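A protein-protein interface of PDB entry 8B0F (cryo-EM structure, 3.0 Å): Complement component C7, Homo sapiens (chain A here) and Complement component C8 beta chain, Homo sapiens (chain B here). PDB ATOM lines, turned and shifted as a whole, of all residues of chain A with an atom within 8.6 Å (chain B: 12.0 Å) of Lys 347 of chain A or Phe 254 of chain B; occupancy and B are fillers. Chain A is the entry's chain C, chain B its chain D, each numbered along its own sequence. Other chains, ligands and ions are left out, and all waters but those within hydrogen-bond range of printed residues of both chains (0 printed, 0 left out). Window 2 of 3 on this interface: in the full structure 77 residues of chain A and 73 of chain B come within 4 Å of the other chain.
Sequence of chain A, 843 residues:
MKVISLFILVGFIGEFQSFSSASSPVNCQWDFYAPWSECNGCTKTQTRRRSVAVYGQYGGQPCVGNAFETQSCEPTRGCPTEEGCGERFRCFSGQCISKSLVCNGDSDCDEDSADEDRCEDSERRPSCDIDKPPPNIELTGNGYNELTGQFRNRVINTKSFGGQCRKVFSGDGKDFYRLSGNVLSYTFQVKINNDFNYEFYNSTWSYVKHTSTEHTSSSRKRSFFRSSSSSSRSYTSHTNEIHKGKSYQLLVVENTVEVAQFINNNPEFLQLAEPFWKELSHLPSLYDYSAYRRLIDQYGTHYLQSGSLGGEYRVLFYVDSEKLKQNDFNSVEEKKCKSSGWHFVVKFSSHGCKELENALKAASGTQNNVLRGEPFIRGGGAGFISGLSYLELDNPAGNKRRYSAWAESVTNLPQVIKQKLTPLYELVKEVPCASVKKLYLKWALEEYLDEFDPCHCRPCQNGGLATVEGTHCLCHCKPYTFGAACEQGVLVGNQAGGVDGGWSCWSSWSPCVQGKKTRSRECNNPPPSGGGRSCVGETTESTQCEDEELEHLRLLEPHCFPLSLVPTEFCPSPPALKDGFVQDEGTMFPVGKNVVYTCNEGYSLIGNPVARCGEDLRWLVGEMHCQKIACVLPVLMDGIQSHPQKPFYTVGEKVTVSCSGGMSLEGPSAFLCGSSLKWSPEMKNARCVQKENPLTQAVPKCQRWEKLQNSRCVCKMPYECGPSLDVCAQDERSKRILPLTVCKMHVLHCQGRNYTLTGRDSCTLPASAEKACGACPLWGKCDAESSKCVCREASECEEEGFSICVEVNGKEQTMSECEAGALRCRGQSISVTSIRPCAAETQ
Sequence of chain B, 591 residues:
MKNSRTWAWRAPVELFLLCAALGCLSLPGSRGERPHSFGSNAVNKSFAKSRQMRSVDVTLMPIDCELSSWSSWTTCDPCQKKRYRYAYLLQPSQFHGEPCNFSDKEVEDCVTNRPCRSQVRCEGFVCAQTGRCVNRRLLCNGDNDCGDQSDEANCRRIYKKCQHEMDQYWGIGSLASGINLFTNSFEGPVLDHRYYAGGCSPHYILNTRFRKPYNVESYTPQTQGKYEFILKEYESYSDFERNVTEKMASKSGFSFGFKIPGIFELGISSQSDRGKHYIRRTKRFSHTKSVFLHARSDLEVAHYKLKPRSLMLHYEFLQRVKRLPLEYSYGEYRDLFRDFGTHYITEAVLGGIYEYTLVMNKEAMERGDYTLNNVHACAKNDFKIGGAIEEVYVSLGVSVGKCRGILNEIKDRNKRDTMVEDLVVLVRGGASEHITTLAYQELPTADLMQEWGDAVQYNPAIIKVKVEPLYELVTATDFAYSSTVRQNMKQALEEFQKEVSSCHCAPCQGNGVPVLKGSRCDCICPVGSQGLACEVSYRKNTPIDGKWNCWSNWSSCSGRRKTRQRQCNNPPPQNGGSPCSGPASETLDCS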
ATOM      1  N   GLY A 341      14.048   8.790 -12.691  1.00  0.00           N
ATOM      2  CA  GLY A 341      15.370   8.924 -13.267  1.00  0.00           C
ATOM      3  C   GLY A 341      15.507   8.137 -14.555  1.00  0.00           C
ATOM      4  O   GLY A 341      14.780   7.173 -14.808  1.00  0.00           O
ATOM      5  N   TRP A 342      16.467   8.573 -15.372  1.00  0.00           N
ATOM      6  CA  TRP A 342      16.707   8.033 -16.705  1.00  0.00           C
ATOM      7  C   TRP A 342      18.191   7.739 -16.863  1.00  0.00           C
ATOM      8  O   TRP A 342      19.037   8.481 -16.356  1.00  0.00           O
ATOM      9  CB  TRP A 342      16.266   9.001 -17.815  1.00  0.00           C
ATOM     10  CG  TRP A 342      14.782   9.179 -17.959  1.00  0.00           C
ATOM     11  CD1 TRP A 342      13.999   8.689 -18.962  1.00  0.00           C
ATOM     12  CD2 TRP A 342      13.905   9.891 -17.077  1.00  0.00           C
ATOM     13  NE1 TRP A 342      12.691   9.058 -18.767  1.00  0.00           N
ATOM     14  CE2 TRP A 342      12.605   9.790 -17.613  1.00  0.00           C
ATOM     15  CE3 TRP A 342      14.088  10.592 -15.883  1.00  0.00           C
ATOM     16  CZ2 TRP A 342      11.498  10.372 -16.999  1.00  0.00           C
ATOM     17  CZ3 TRP A 342      12.988  11.167 -15.274  1.00  0.00           C
ATOM     18  CH2 TRP A 342      11.711  11.055 -15.834  1.00  0.00           C
ATOM     19  N   HIS A 343      18.500   6.650 -17.569  1.00  0.00           N
ATOM     20  CA  HIS A 343      19.882   6.301 -17.872  1.00  0.00           C
ATOM     21  C   HIS A 343      20.122   5.877 -19.313  1.00  0.00           C
ATOM     22  O   HIS A 343      21.249   5.485 -19.633  1.00  0.00           O
ATOM     23  CB  HIS A 343      20.366   5.186 -16.931  1.00  0.00           C
ATOM     24  CG  HIS A 343      20.162   5.493 -15.481  1.00  0.00           C
ATOM     25  ND1 HIS A 343      18.940   5.369 -14.858  1.00  0.00           N
ATOM     26  CD2 HIS A 343      21.026   5.925 -14.533  1.00  0.00           C
ATOM     27  CE1 HIS A 343      19.060   5.709 -13.587  1.00  0.00           C
ATOM     28  NE2 HIS A 343      20.316   6.050 -13.364  1.00  0.00           N
ATOM     29  N   PHE A 344      19.121   5.939 -20.192  1.00  0.00           N
ATOM     30  CA  PHE A 344      19.222   5.342 -21.517  1.00  0.00           C
ATOM     31  C   PHE A 344      19.136   6.366 -22.639  1.00  0.00           C
ATOM     32  O   PHE A 344      19.182   5.980 -23.813  1.00  0.00           O
ATOM     33  CB  PHE A 344      18.127   4.281 -21.707  1.00  0.00           C
ATOM     34  CG  PHE A 344      16.764   4.854 -21.974  1.00  0.00           C
ATOM     35  CD1 PHE A 344      15.941   5.237 -20.928  1.00  0.00           C
ATOM     36  CD2 PHE A 344      16.298   4.996 -23.272  1.00  0.00           C
ATOM     37  CE1 PHE A 344      14.684   5.759 -21.171  1.00  0.00           C
ATOM     38  CE2 PHE A 344      15.043   5.518 -23.521  1.00  0.00           C
ATOM     39  CZ  PHE A 344      14.235   5.898 -22.469  1.00  0.00           C
ATOM     40  N   VAL A 345      19.012   7.653 -22.317  1.00  0.00           N
ATOM     41  CA  VAL A 345      19.117   8.718 -23.307  1.00  0.00           C
ATOM     42  C   VAL A 345      20.169   9.698 -22.810  1.00  0.00           C
ATOM     43  O   VAL A 345      21.195   9.916 -23.464  1.00  0.00           O
ATOM     44  CB  VAL A 345      17.765   9.418 -23.539  1.00  0.00           C
ATOM     45  CG1 VAL A 345      17.896  10.497 -24.607  1.00  0.00           C
ATOM     46  CG2 VAL A 345      16.701   8.404 -23.925  1.00  0.00           C
ATOM     47  N   VAL A 346      19.916  10.293 -21.647  1.00  0.00           N
ATOM     48  CA  VAL A 346      20.917  11.045 -20.901  1.00  0.00           C
ATOM     49  C   VAL A 346      20.808  10.638 -19.439  1.00  0.00           C
ATOM     50  O   VAL A 346      19.703  10.522 -18.899  1.00  0.00           O
ATOM     51  CB  VAL A 346      20.736  12.568 -21.074  1.00  0.00           C
ATOM     52  CG1 VAL A 346      21.685  13.334 -20.158  1.00  0.00           C
ATOM     53  CG2 VAL A 346      20.954  12.965 -22.526  1.00  0.00           C
ATOM     54  N   LYS A 347      21.954  10.421 -18.796  1.00  0.00           N
ATOM     55  CA  LYS A 347      21.972  10.083 -17.379  1.00  0.00           C
ATOM     56  C   LYS A 347      21.439  11.238 -16.541  1.00  0.00           C
ATOM     57  O   LYS A 347      22.068  12.298 -16.461  1.00  0.00           O
ATOM     58  CB  LYS A 347      23.391   9.709 -16.945  1.00  0.00           C
ATOM     59  CG  LYS A 347      23.889   8.402 -17.551  1.00  0.00           C
ATOM     60  CD  LYS A 347      25.184   7.923 -16.909  1.00  0.00           C
ATOM     61  CE  LYS A 347      26.327   8.901 -17.142  1.00  0.00           C
ATOM     62  NZ  LYS A 347      27.605   8.413 -16.552  1.00  0.00           N
ATOM     63  N   PHE A 348      20.280  11.041 -15.913  1.00  0.00           N
ATOM     64  CA  PHE A 348      19.522  12.136 -15.327  1.00  0.00           C
ATOM     65  C   PHE A 348      18.806  11.629 -14.082  1.00  0.00           C
ATOM     66  O   PHE A 348      18.437  10.454 -13.999  1.00  0.00           O
ATOM     67  CB  PHE A 348      18.529  12.708 -16.350  1.00  0.00           C
ATOM     68  CG  PHE A 348      17.420  13.519 -15.745  1.00  0.00           C
ATOM     69  CD1 PHE A 348      17.694  14.661 -15.014  1.00  0.00           C
ATOM     70  CD2 PHE A 348      16.101  13.149 -15.928  1.00  0.00           C
ATOM     71  CE1 PHE A 348      16.672  15.411 -14.466  1.00  0.00           C
ATOM     72  CE2 PHE A 348      15.074  13.892 -15.382  1.00  0.00           C
ATOM     73  CZ  PHE A 348      15.361  15.025 -14.650  1.00  0.00           C
ATOM     74  N   SER A 349      18.610  12.525 -13.114  1.00  0.00           N
ATOM     75  CA  SER A 349      17.921  12.200 -11.873  1.00  0.00           C
ATOM     76  C   SER A 349      17.073  13.384 -11.429  1.00  0.00           C
ATOM     77  O   SER A 349      17.444  14.543 -11.631  1.00  0.00           O
ATOM     78  CB  SER A 349      18.911  11.824 -10.764  1.00  0.00           C
ATOM     79  OG  SER A 349      18.242  11.599  -9.536  1.00  0.00           O
ATOM     80  N   SER A 350      15.925  13.080 -10.823  1.00  0.00           N
ATOM     81  CA  SER A 350      15.057  14.098 -10.246  1.00  0.00           C
ATOM     82  C   SER A 350      14.361  13.534  -9.014  1.00  0.00           C
ATOM     83  O   SER A 350      14.004  12.354  -8.985  1.00  0.00           O
ATOM     84  CB  SER A 350      14.018  14.585 -11.262  1.00  0.00           C
ATOM     85  OG  SER A 350      13.180  13.523 -11.682  1.00  0.00           O
ATOM     86  N   SER B 250      13.604  19.494  -3.129  1.00  0.00           N
ATOM     87  CA  SER B 250      13.746  19.158  -4.539  1.00  0.00           C
ATOM     88  C   SER B 250      15.215  18.936  -4.871  1.00  0.00           C
ATOM     89  O   SER B 250      16.081  19.690  -4.418  1.00  0.00           O
ATOM     90  CB  SER B 250      13.170  20.262  -5.434  1.00  0.00           C
ATOM     91  OG  SER B 250      13.282  19.916  -6.804  1.00  0.00           O
ATOM     92  N   LYS B 251      15.493  17.896  -5.659  1.00  0.00           N
ATOM     93  CA  LYS B 251      16.818  17.670  -6.218  1.00  0.00           C
ATOM     94  C   LYS B 251      16.699  17.330  -7.697  1.00  0.00           C
ATOM     95  O   LYS B 251      15.686  16.790  -8.149  1.00  0.00           O
ATOM     96  CB  LYS B 251      17.590  16.555  -5.493  1.00  0.00           C
ATOM     97  CG  LYS B 251      17.632  16.695  -3.980  1.00  0.00           C
ATOM     98  CD  LYS B 251      18.693  15.787  -3.357  1.00  0.00           C
ATOM     99  CE  LYS B 251      18.447  14.306  -3.615  1.00  0.00           C
ATOM    100  NZ  LYS B 251      17.309  13.776  -2.816  1.00  0.00           N
ATOM    101  N   SER B 252      17.750  17.660  -8.445  1.00  0.00           N
ATOM    102  CA  SER B 252      17.872  17.267  -9.842  1.00  0.00           C
ATOM    103  C   SER B 252      19.351  17.181 -10.186  1.00  0.00           C
ATOM    104  O   SER B 252      20.186  17.828  -9.550  1.00  0.00           O
ATOM    105  CB  SER B 252      17.168  18.255 -10.781  1.00  0.00           C
ATOM    106  OG  SER B 252      15.771  18.293 -10.547  1.00  0.00           O
ATOM    107  N   GLY B 253      19.669  16.377 -11.194  1.00  0.00           N
ATOM    108  CA  GLY B 253      21.043  16.275 -11.646  1.00  0.00           C
ATOM    109  C   GLY B 253      21.157  15.477 -12.922  1.00  0.00           C
ATOM    110  O   GLY B 253      20.242  14.740 -13.306  1.00  0.00           O
ATOM    111  N   PHE B 254      22.305  15.633 -13.575  1.00  0.00           N
ATOM    112  CA  PHE B 254      22.543  15.064 -14.898  1.00  0.00           C
ATOM    113  C   PHE B 254      23.936  14.448 -14.966  1.00  0.00           C
ATOM    114  O   PHE B 254      24.729  14.580 -14.035  1.00  0.00           O
ATOM    115  CB  PHE B 254      22.405  16.133 -15.986  1.00  0.00           C
ATOM    116  CG  PHE B 254      21.026  16.713 -16.103  1.00  0.00           C
ATOM    117  CD1 PHE B 254      20.604  17.717 -15.249  1.00  0.00           C
ATOM    118  CD2 PHE B 254      20.157  16.266 -17.084  1.00  0.00           C
ATOM    119  CE1 PHE B 254      19.337  18.255 -15.363  1.00  0.00           C
ATOM    120  CE2 PHE B 254      18.889  16.801 -17.203  1.00  0.00           C
ATOM    121  CZ  PHE B 254      18.479  17.796 -16.341  1.00  0.00           C
ATOM    122  N   SER B 269      26.859  17.007 -16.481  1.00  0.00           N
ATOM    123  CA  SER B 269      26.998  17.001 -15.029  1.00  0.00           C
ATOM    124  C   SER B 269      26.419  18.275 -14.425  1.00  0.00           C
ATOM    125  O   SER B 269      26.954  19.366 -14.625  1.00  0.00           O
ATOM    126  CB  SER B 269      28.468  16.850 -14.633  1.00  0.00           C
ATOM    127  OG  SER B 269      28.631  16.941 -13.229  1.00  0.00           O
ATOM    128  N   SER B 270      25.321  18.132 -13.683  1.00  0.00           N
ATOM    129  CA  SER B 270      24.679  19.269 -13.044  1.00  0.00           C
ATOM    130  C   SER B 270      23.976  18.800 -11.778  1.00  0.00           C
ATOM    131  O   SER B 270      23.652  17.621 -11.623  1.00  0.00           O
ATOM    132  CB  SER B 270      23.682  19.955 -13.986  1.00  0.00           C
ATOM    133  OG  SER B 270      23.261  21.203 -13.463  1.00  0.00           O
ATOM    134  N   GLN B 271      23.766  19.744 -10.862  1.00  0.00           N
ATOM    135  CA  GLN B 271      22.997  19.516  -9.646  1.00  0.00           C
ATOM    136  C   GLN B 271      22.118  20.730  -9.385  1.00  0.00           C
ATOM    137  O   GLN B 271      22.474  21.857  -9.737  1.00  0.00           O
ATOM    138  CB  GLN B 271      23.904  19.236  -8.440  1.00  0.00           C
ATOM    139  CG  GLN B 271      25.080  18.323  -8.753  1.00  0.00           C
ATOM    140  CD  GLN B 271      25.962  18.068  -7.549  1.00  0.00           C
ATOM    141  OE1 GLN B 271      25.546  18.265  -6.407  1.00  0.00           O
ATOM    142  NE2 GLN B 271      27.189  17.626  -7.797  1.00  0.00           N
ATOM    143  N   SER B 272      20.959  20.494  -8.769  1.00  0.00           N
ATOM    144  CA  SER B 272      20.039  21.579  -8.428  1.00  0.00           C
ATOM    145  C   SER B 272      19.217  21.155  -7.218  1.00  0.00           C
ATOM    146  O   SER B 272      18.316  20.321  -7.337  1.00  0.00           O
ATOM    147  CB  SER B 272      19.126  21.924  -9.606  1.00  0.00           C
ATOM    148  OG  SER B 272      19.861  22.302 -10.759  1.00  0.00           O
ATOM    149  N   ASP B 273      19.532  21.737  -6.063  1.00  0.00           N
ATOM    150  CA  ASP B 273      18.866  21.450  -4.799  1.00  0.00           C
ATOM    151  C   ASP B 273      18.030  22.653  -4.385  1.00  0.00           C
ATOM    152  O   ASP B 273      18.508  23.791  -4.442  1.00  0.00           O
ATOM    153  CB  ASP B 273      19.884  21.112  -3.708  1.00  0.00           C
ATOM    154  CG  ASP B 273      20.982  20.193  -4.203  1.00  0.00           C
ATOM    155  OD1 ASP B 273      20.821  19.607  -5.294  1.00  0.00           O
ATOM    156  OD2 ASP B 273      22.007  20.057  -3.502  1.00  0.00           O
ATOM    157  N   CYS B 378      20.652  25.621  -4.043  1.00  0.00           N
ATOM    158  CA  CYS B 378      21.993  25.711  -4.604  1.00  0.00           C
ATOM    159  C   CYS B 378      22.118  24.759  -5.786  1.00  0.00           C
ATOM    160  O   CYS B 378      21.536  23.671  -5.782  1.00  0.00           O
ATOM    161  CB  CYS B 378      23.061  25.402  -3.551  1.00  0.00           C
ATOM    162  SG  CYS B 378      24.705  25.945  -4.045  1.00  0.00           S
ATOM    163  N   ALA B 379      22.883  25.180  -6.792  1.00  0.00           N
ATOM    164  CA  ALA B 379      23.105  24.411  -8.010  1.00  0.00           C
ATOM    165  C   ALA B 379      24.596  24.220  -8.253  1.00  0.00           C
ATOM    166  O   ALA B 379      25.375  25.170  -8.130  1.00  0.00           O
ATOM    167  CB  ALA B 379      22.466  25.105  -9.215  1.00  0.00           C
ATOM    168  N   LYS B 380      24.988  22.993  -8.596  1.00  0.00           N
ATOM    169  CA  LYS B 380      26.386  22.626  -8.789  1.00  0.00           C
ATOM    170  C   LYS B 380      26.547  22.018 -10.173  1.00  0.00           C
ATOM    171  O   LYS B 380      25.766  21.146 -10.567  1.00  0.00           O
ATOM    172  CB  LYS B 380      26.870  21.631  -7.728  1.00  0.00           C
ATOM    173  CG  LYS B 380      26.599  22.036  -6.292  1.00  0.00           C
ATOM    174  CD  LYS B 380      27.386  23.283  -5.921  1.00  0.00           C
ATOM    175  CE  LYS B 380      27.203  23.643  -4.458  1.00  0.00           C
ATOM    176  NZ  LYS B 380      27.809  22.624  -3.558  1.00  0.00           N
ATOM    177  N   ASN B 381      27.558  22.477 -10.906  1.00  0.00           N
ATOM    178  CA  ASN B 381      27.751  22.068 -12.294  1.00  0.00           C
ATOM    179  C   ASN B 381      29.214  21.729 -12.554  1.00  0.00           C
ATOM    180  O   ASN B 381      30.079  21.981 -11.715  1.00  0.00           O
ATOM    181  CB  ASN B 381      27.293  23.172 -13.250  1.00  0.00           C
ATOM    182  CG  ASN B 381      26.025  23.859 -12.783  1.00  0.00           C
ATOM    183  OD1 ASN B 381      24.925  23.333 -12.943  1.00  0.00           O
ATOM    184  ND2 ASN B 381      26.177  25.037 -12.190  1.00  0.00           N
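Lys 347 of chain A touches just one residue of chain B: Phe 254. Of chain A, only Lys 347 (3.2 Å) and Phe 348 (3.3 Å) come within 4 Å of Phe 254 of chain B. No residue of chain B comes within 4 Å of His 343 of chain A. Val 345 of chain A touches none of the printed residues of chain B. No residue of chain B comes within 4 Å of Val 346 of chain A. Of chain B, only Ser 252 and Gly 253 come within 4 Å of Ser 349 of chain A. Of the printed residues of chain A, Gly 253 of chain B touches Phe 348 (3.1 Å) and Ser 349 (2.8 Å). Of the printed residues of chain B, Ser 350 of chain A touches Lys 251. Of the printed residues of chain A, Lys 251 of chain B touches Ser 350. Trp 342 of chain A touches none of the printed residues of chain B. The nearest residue of chain B that does not touch Lys 347 of chain A is Gly 253 of chain B (4.4 Å).
Of the 10 printed residues of chain A, 4 touch a printed residue of chain B. Printed residues of chain A that touch a printed residue of chain B: Lys 347, Phe 348, Ser 349 and Ser 350. Hydrophobic or aromatic side chains of chain A within 4 Å of the printed part of chain B: Phe 348. Hydrophobic or aromatic side chains of chain B within 4 Å of the printed part of chain A: Phe 254. Among the printed residues, 6 pairs touch across the chains.
N of Ser 349 of chain A sits at hydrogen-bond distance from O of Gly 253 of chain B (2.8 Å).
The backbone carbonyl oxygen (O) of Ser 252 of chain B sits at hydrogen-bond distance from the backbone NH (N) of Ser 272 of chain B, at 2.9 Å. N of Phe 348 of chain A sits at hydrogen-bond distance from O of Trp 342 of chain A, 2.9 Å away. The backbone NH (N) of Phe 254 of chain B sits at hydrogen-bond distance from the backbone carbonyl oxygen (O) of Ser 270 of chain B.
Among the printed residues, pairs that only touch across the chains: Lys 347 of chain A with Phe 254 of chain B (3.2 Å), Phe 348 of chain A with Gly 253 of chain B (3.1 Å), Phe 348 of chain A with Phe 254 of chain B (3.3 Å), Ser 349 of chain A with Ser 252 of chain B (3.3 Å) and Ser 350 of chain A with Lys 251 of chain B (3.5 Å).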
